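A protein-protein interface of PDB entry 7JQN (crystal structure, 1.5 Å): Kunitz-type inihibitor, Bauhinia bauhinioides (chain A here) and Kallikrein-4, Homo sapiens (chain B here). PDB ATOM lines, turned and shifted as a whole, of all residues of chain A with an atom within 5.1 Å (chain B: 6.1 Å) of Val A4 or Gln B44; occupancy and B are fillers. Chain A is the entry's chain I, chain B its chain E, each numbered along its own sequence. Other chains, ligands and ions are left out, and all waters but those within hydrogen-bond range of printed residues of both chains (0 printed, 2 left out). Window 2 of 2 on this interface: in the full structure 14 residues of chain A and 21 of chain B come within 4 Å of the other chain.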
ATOM      1  N   SER A   2      31.470  -1.370 -30.141  1.00  0.00           N
ATOM      2  CA  SER A   2      30.888  -0.044 -30.038  1.00  0.00           C
ATOM      3  C   SER A   2      30.504   0.251 -28.587  1.00  0.00           C
ATOM      4  O   SER A   2      30.144   1.377 -28.231  1.00  0.00           O
ATOM      5  CB  SER A   2      29.723   0.099 -30.970  1.00  0.00           C
ATOM      6  OG  SER A   2      28.514  -0.392 -30.381  1.00  0.00           O
ATOM      7  N   SER A   3      30.572  -0.798 -27.773  1.00  0.00           N
ATOM      8  CA  SER A   3      30.368  -0.690 -26.346  1.00  0.00           C
ATOM      9  C   SER A   3      31.350   0.294 -25.724  1.00  0.00           C
ATOM     10  O   SER A   3      32.555   0.316 -26.005  1.00  0.00           O
ATOM     11  CB  SER A   3      30.504  -2.015 -25.683  1.00  0.00           C
ATOM     12  OG  SER A   3      29.348  -2.792 -25.962  1.00  0.00           O
ATOM     13  N   VAL A   4      30.784   1.130 -24.874  1.00  0.00           N
ATOM     14  CA  VAL A   4      31.534   2.037 -24.040  1.00  0.00           C
ATOM     15  C   VAL A   4      32.145   1.245 -22.879  1.00  0.00           C
ATOM     16  O   VAL A   4      31.487   0.417 -22.227  1.00  0.00           O
ATOM     17  CB  VAL A   4      30.598   3.154 -23.583  1.00  0.00           C
ATOM     18  CG1 VAL A   4      31.218   4.103 -22.578  1.00  0.00           C
ATOM     19  CG2 VAL A   4      30.028   3.886 -24.791  1.00  0.00           C
ATOM     20  N   VAL A   5      33.424   1.487 -22.618  1.00  0.00           N
ATOM     21  CA  VAL A   5      34.086   0.881 -21.466  1.00  0.00           C
ATOM     22  C   VAL A   5      33.601   1.599 -20.209  1.00  0.00           C
ATOM     23  O   VAL A   5      33.640   2.838 -20.144  1.00  0.00           O
ATOM     24  CB  VAL A   5      35.623   1.010 -21.585  1.00  0.00           C
ATOM     25  CG1 VAL A   5      36.321   0.425 -20.356  1.00  0.00           C
ATOM     26  CG2 VAL A   5      36.134   0.339 -22.885  1.00  0.00           C
ATOM     27  N   VAL A   6      33.146   0.824 -19.197  1.00  0.00           N
ATOM     28  CA  VAL A   6      32.639   1.422 -17.963  1.00  0.00           C
ATOM     29  C   VAL A   6      33.456   0.962 -16.753  1.00  0.00           C
ATOM     30  O   VAL A   6      34.064  -0.121 -16.744  1.00  0.00           O
ATOM     31  CB  VAL A   6      31.139   1.136 -17.753  1.00  0.00           C
ATOM     32  CG1 VAL A   6      30.309   1.751 -18.873  1.00  0.00           C
ATOM     33  CG2 VAL A   6      30.848  -0.357 -17.602  1.00  0.00           C
ATOM     34  N   PRO A  12      30.987   5.724 -17.695  1.00  0.00           N
ATOM     35  CA  PRO A  12      31.979   5.626 -18.779  1.00  0.00           C
ATOM     36  C   PRO A  12      33.362   5.997 -18.245  1.00  0.00           C
ATOM     37  O   PRO A  12      33.520   6.989 -17.515  1.00  0.00           O
ATOM     38  CB  PRO A  12      31.517   6.721 -19.767  1.00  0.00           C
ATOM     39  CG  PRO A  12      29.998   6.785 -19.529  1.00  0.00           C
ATOM     40  CD  PRO A  12      29.856   6.624 -18.017  1.00  0.00           C
ATOM     41  N   ILE A  68      34.926   9.880 -23.674  1.00  0.00           N
ATOM     42  CA  ILE A  68      34.698   8.505 -23.223  1.00  0.00           C
ATOM     43  C   ILE A  68      35.539   7.567 -24.086  1.00  0.00           C
ATOM     44  O   ILE A  68      36.059   7.966 -25.141  1.00  0.00           O
ATOM     45  CB  ILE A  68      33.200   8.119 -23.298  1.00  0.00           C
ATOM     46  CG1 ILE A  68      32.683   8.101 -24.742  1.00  0.00           C
ATOM     47  CG2 ILE A  68      32.353   8.988 -22.367  1.00  0.00           C
ATOM     48  CD1 ILE A  68      31.238   7.652 -24.898  1.00  0.00           C
ATOM     49  N   ILE A  69      35.669   6.317 -23.652  1.00  0.00           N
ATOM     50  CA  ILE A  69      36.453   5.304 -24.352  1.00  0.00           C
ATOM     51  C   ILE A  69      35.527   4.155 -24.750  1.00  0.00           C
ATOM     52  O   ILE A  69      34.723   3.686 -23.928  1.00  0.00           O
ATOM     53  CB  ILE A  69      37.547   4.790 -23.387  1.00  0.00           C
ATOM     54  CG1 ILE A  69      38.503   5.931 -23.012  1.00  0.00           C
ATOM     55  CG2 ILE A  69      38.247   3.557 -23.935  1.00  0.00           C
ATOM     56  CD1 ILE A  69      39.220   6.528 -24.167  1.00  0.00           C
ATOM     57  N   LYS A  70      35.629   3.723 -26.008  1.00  0.00           N
ATOM     58  CA  LYS A  70      34.941   2.551 -26.535  1.00  0.00           C
ATOM     59  C   LYS A  70      35.924   1.389 -26.660  1.00  0.00           C
ATOM     60  O   LYS A  70      37.142   1.585 -26.846  1.00  0.00           O
ATOM     61  CB  LYS A  70      34.298   2.878 -27.896  1.00  0.00           C
ATOM     62  CG  LYS A  70      33.073   3.813 -27.752  1.00  0.00           C
ATOM     63  CD  LYS A  70      32.424   4.424 -28.992  1.00  0.00           C
ATOM     64  CE  LYS A  70      32.644   3.615 -30.235  1.00  0.00           C
ATOM     65  NZ  LYS A  70      31.858   4.149 -31.380  1.00  0.00           N
ATOM     66  N   GLU A  71      35.383   0.156 -26.637  1.00  0.00           N
ATOM     67  CA  GLU A  71      36.229  -1.027 -26.729  1.00  0.00           C
ATOM     68  C   GLU A  71      36.984  -1.089 -28.059  1.00  0.00           C
ATOM     69  O   GLU A  71      38.049  -1.729 -28.129  1.00  0.00           O
ATOM     70  CB  GLU A  71      35.383  -2.295 -26.586  1.00  0.00           C
ATOM     71  CG  GLU A  71      34.850  -2.449 -25.179  1.00  0.00           C
ATOM     72  CD  GLU A  71      34.047  -3.734 -25.008  1.00  0.00           C
ATOM     73  OE1 GLU A  71      34.462  -4.785 -25.573  1.00  0.00           O
ATOM     74  OE2 GLU A  71      33.024  -3.695 -24.265  1.00  0.00           O
ATOM     75  N   TYR A 122      37.164  -6.911 -18.106  1.00  0.00           N
ATOM     76  CA  TYR A 122      37.822  -6.495 -19.338  1.00  0.00           C
ATOM     77  C   TYR A 122      39.209  -7.117 -19.380  1.00  0.00           C
ATOM     78  O   TYR A 122      39.822  -7.367 -18.342  1.00  0.00           O
ATOM     79  CB  TYR A 122      38.026  -4.967 -19.386  1.00  0.00           C
ATOM     80  CG  TYR A 122      36.740  -4.198 -19.513  1.00  0.00           C
ATOM     81  CD1 TYR A 122      36.096  -4.116 -20.740  1.00  0.00           C
ATOM     82  CD2 TYR A 122      36.116  -3.624 -18.396  1.00  0.00           C
ATOM     83  CE1 TYR A 122      34.871  -3.461 -20.871  1.00  0.00           C
ATOM     84  CE2 TYR A 122      34.919  -2.929 -18.527  1.00  0.00           C
ATOM     85  CZ  TYR A 122      34.288  -2.863 -19.763  1.00  0.00           C
ATOM     86  OH  TYR A 122      33.101  -2.191 -19.881  1.00  0.00           O
ATOM     87  N   MET B  20      23.862  10.470 -23.759  1.00  0.00           N
ATOM     88  CA  MET B  20      23.866   9.091 -23.268  1.00  0.00           C
ATOM     89  C   MET B  20      23.658   9.211 -21.770  1.00  0.00           C
ATOM     90  O   MET B  20      24.459   9.871 -21.095  1.00  0.00           O
ATOM     91  CB  MET B  20      25.263   8.516 -23.587  1.00  0.00           C
ATOM     92  CG  MET B  20      25.622   7.110 -23.135  1.00  0.00           C
ATOM     93  SD  MET B  20      27.435   6.827 -23.416  1.00  0.00           S
ATOM     94  CE  MET B  20      27.537   6.798 -25.203  1.00  0.00           C
ATOM     95  N   PHE B  25      28.033  13.173 -25.058  1.00  0.00           N
ATOM     96  CA  PHE B  25      29.303  12.531 -25.362  1.00  0.00           C
ATOM     97  C   PHE B  25      29.875  12.974 -26.705  1.00  0.00           C
ATOM     98  O   PHE B  25      31.076  12.817 -26.910  1.00  0.00           O
ATOM     99  CB  PHE B  25      29.239  11.005 -25.289  1.00  0.00           C
ATOM    100  CG  PHE B  25      28.358  10.375 -26.335  1.00  0.00           C
ATOM    101  CD1 PHE B  25      26.980  10.319 -26.169  1.00  0.00           C
ATOM    102  CD2 PHE B  25      28.912   9.852 -27.493  1.00  0.00           C
ATOM    103  CE1 PHE B  25      26.178   9.709 -27.136  1.00  0.00           C
ATOM    104  CE2 PHE B  25      28.119   9.275 -28.472  1.00  0.00           C
ATOM    105  CZ  PHE B  25      26.740   9.194 -28.294  1.00  0.00           C
ATOM    106  N   CYS B  42      31.864   8.365 -33.046  1.00  0.00           N
ATOM    107  CA  CYS B  42      30.801   8.581 -32.069  1.00  0.00           C
ATOM    108  C   CYS B  42      29.674   7.553 -32.230  1.00  0.00           C
ATOM    109  O   CYS B  42      28.649   7.646 -31.526  1.00  0.00           O
ATOM    110  CB  CYS B  42      30.203   9.975 -32.217  1.00  0.00           C
ATOM    111  SG  CYS B  42      31.402  11.290 -31.845  1.00  0.00           S
ATOM    112  N   PHE B  43      29.849   6.558 -33.115  1.00  0.00           N
ATOM    113  CA  PHE B  43      28.809   5.568 -33.415  1.00  0.00           C
ATOM    114  C   PHE B  43      28.286   4.880 -32.149  1.00  0.00           C
ATOM    115  O   PHE B  43      29.070   4.440 -31.295  1.00  0.00           O
ATOM    116  CB  PHE B  43      29.323   4.514 -34.407  1.00  0.00           C
ATOM    117  CG  PHE B  43      28.332   3.394 -34.618  1.00  0.00           C
ATOM    118  CD1 PHE B  43      27.359   3.499 -35.596  1.00  0.00           C
ATOM    119  CD2 PHE B  43      28.368   2.239 -33.830  1.00  0.00           C
ATOM    120  CE1 PHE B  43      26.443   2.472 -35.786  1.00  0.00           C
ATOM    121  CE2 PHE B  43      27.432   1.223 -34.003  1.00  0.00           C
ATOM    122  CZ  PHE B  43      26.470   1.351 -34.979  1.00  0.00           C
ATOM    123  N   GLN B  44      26.953   4.773 -32.064  1.00  0.00           N
ATOM    124  CA  GLN B  44      26.289   3.935 -31.071  1.00  0.00           C
ATOM    125  C   GLN B  44      25.141   3.215 -31.768  1.00  0.00           C
ATOM    126  O   GLN B  44      24.672   3.683 -32.798  1.00  0.00           O
ATOM    127  CB  GLN B  44      25.716   4.772 -29.920  1.00  0.00           C
ATOM    128  CG  GLN B  44      26.798   5.387 -29.015  1.00  0.00           C
ATOM    129  CD  GLN B  44      27.438   4.337 -28.118  1.00  0.00           C
ATOM    130  OE1 GLN B  44      26.898   3.991 -27.046  1.00  0.00           O
ATOM    131  NE2 GLN B  44      28.575   3.787 -28.540  1.00  0.00           N
ATOM    132  N   ASN B  45      24.589   2.166 -31.121  1.00  0.00           N
ATOM    133  CA  ASN B  45      23.494   1.435 -31.733  1.00  0.00           C
ATOM    134  C   ASN B  45      22.186   2.235 -31.728  1.00  0.00           C
ATOM    135  O   ASN B  45      21.314   1.965 -32.539  1.00  0.00           O
ATOM    136  CB  ASN B  45      23.308   0.090 -31.048  1.00  0.00           C
ATOM    137  CG  ASN B  45      24.401  -0.887 -31.424  1.00  0.00           C
ATOM    138  OD1 ASN B  45      24.760  -0.994 -32.591  1.00  0.00           O
ATOM    139  ND2 ASN B  45      24.917  -1.614 -30.448  1.00  0.00           N
ATOM    140  N   SER B  46      22.060   3.217 -30.833  1.00  0.00           N
ATOM    141  CA  SER B  46      20.922   4.135 -30.851  1.00  0.00           C
ATOM    142  C   SER B  46      21.367   5.447 -30.221  1.00  0.00           C
ATOM    143  O   SER B  46      22.394   5.491 -29.531  1.00  0.00           O
ATOM    144  CB  SER B  46      19.714   3.576 -30.132  1.00  0.00           C
ATOM    145  OG  SER B  46      20.035   3.364 -28.764  1.00  0.00           O
ATOM    146  N   TYR B  47      20.571   6.501 -30.442  1.00  0.00           N
ATOM    147  CA  TYR B  47      20.918   7.838 -29.979  1.00  0.00           C
ATOM    148  C   TYR B  47      19.701   8.564 -29.411  1.00  0.00           C
ATOM    149  O   TYR B  47      18.559   8.340 -29.841  1.00  0.00           O
ATOM    150  CB  TYR B  47      21.438   8.716 -31.127  1.00  0.00           C
ATOM    151  CG  TYR B  47      22.535   8.077 -31.958  1.00  0.00           C
ATOM    152  CD1 TYR B  47      22.229   7.267 -33.033  1.00  0.00           C
ATOM    153  CD2 TYR B  47      23.879   8.289 -31.662  1.00  0.00           C
ATOM    154  CE1 TYR B  47      23.218   6.652 -33.792  1.00  0.00           C
ATOM    155  CE2 TYR B  47      24.890   7.704 -32.420  1.00  0.00           C
ATOM    156  CZ  TYR B  47      24.550   6.894 -33.487  1.00  0.00           C
ATOM    157  OH  TYR B  47      25.544   6.304 -34.218  1.00  0.00           O
ATOM    158  N   SER B  70      17.562   5.457 -34.366  1.00  0.00           N
ATOM    159  CA  SER B  70      18.060   4.078 -34.307  1.00  0.00           C
ATOM    160  C   SER B  70      19.145   3.828 -35.361  1.00  0.00           C
ATOM    161  O   SER B  70      20.124   3.128 -35.120  1.00  0.00           O
ATOM    162  CB  SER B  70      16.931   3.048 -34.475  1.00  0.00           C
ATOM    163  OG  SER B  70      15.712   3.548 -33.965  1.00  0.00           O
ATOM    164  N   SER B  72      22.105   4.397 -38.049  1.00  0.00           N
ATOM    165  CA  SER B  72      23.168   5.270 -38.508  1.00  0.00           C
ATOM    166  C   SER B  72      24.070   4.487 -39.458  1.00  0.00           C
ATOM    167  O   SER B  72      24.061   3.247 -39.438  1.00  0.00           O
ATOM    168  CB  SER B  72      23.887   5.982 -37.361  1.00  0.00           C
ATOM    169  OG  SER B  72      24.477   5.062 -36.470  1.00  0.00           O
ATOM    170  N   MET B  88      29.765   9.808 -40.157  1.00  0.00           N
ATOM    171  CA  MET B  88      28.597   8.934 -40.200  1.00  0.00           C
ATOM    172  C   MET B  88      27.338   9.788 -40.324  1.00  0.00           C
ATOM    173  O   MET B  88      27.322  10.965 -39.940  1.00  0.00           O
ATOM    174  CB  MET B  88      28.501   8.052 -38.945  1.00  0.00           C
ATOM    175  CG  MET B  88      28.186   8.796 -37.683  1.00  0.00           C
ATOM    176  SD  MET B  88      27.900   7.556 -36.372  1.00  0.00           S
ATOM    177  CE  MET B  88      27.650   8.730 -35.030  1.00  0.00           C
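O of Phe B43 sits at hydrogen-bond distance from NZ of Lys A70 (2.8 Å). O of Ser A2 sits at hydrogen-bond distance from NE2 of Gln B44, 2.9 Å away.
Ser A2 touches Phe B43. Ser A2 touches Asn B45 (OG to ND2, 3.8 Å). Met B20 touches Val A4. Val A4 touches Gln B44. Ile A68 touches Met B20. CB of Phe B25 touches CD1 of Ile A68 (3.9 Å). Lys A70 touches Gln B44 (CD to NE2, 3.9 Å).
Of the 11 printed residues of chain A, 4 touch a printed residue of chain B. Hydrophobic or aromatic side chains of chain A within 4 Å of the printed part of chain B: Val A4 and Ile A68. Of the 11 printed residues of chain B, 5 touch a printed residue of chain A.
Val A4 touches just these residues of chain B: Met B20 (3.9 Å) and Gln B44 (3.9 Å). Gln B44 touches just these residues of chain A: Ser A2 (2.9 Å), Val A4 (3.9 Å) and Lys A70 (3.9 Å). Of the printed residues of chain A, Phe B43 touches Ser A2 and Lys A70. Of the printed residues of chain A, Asn B45 touches Ser A2. Of the printed residues of chain A, Phe B25 touches Ile A68. Ser B70 touches none of the printed residues of chain A. The nearest printed residue of chain B that does not touch Val A4 is Phe B43 (6.6 Å). The nearest printed residue of chain A that does not touch Asn B45 is Ser A3 (6.3 Å).
N of Gln B44 sits at hydrogen-bond distance from OH of Tyr B47 (3.0 Å).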
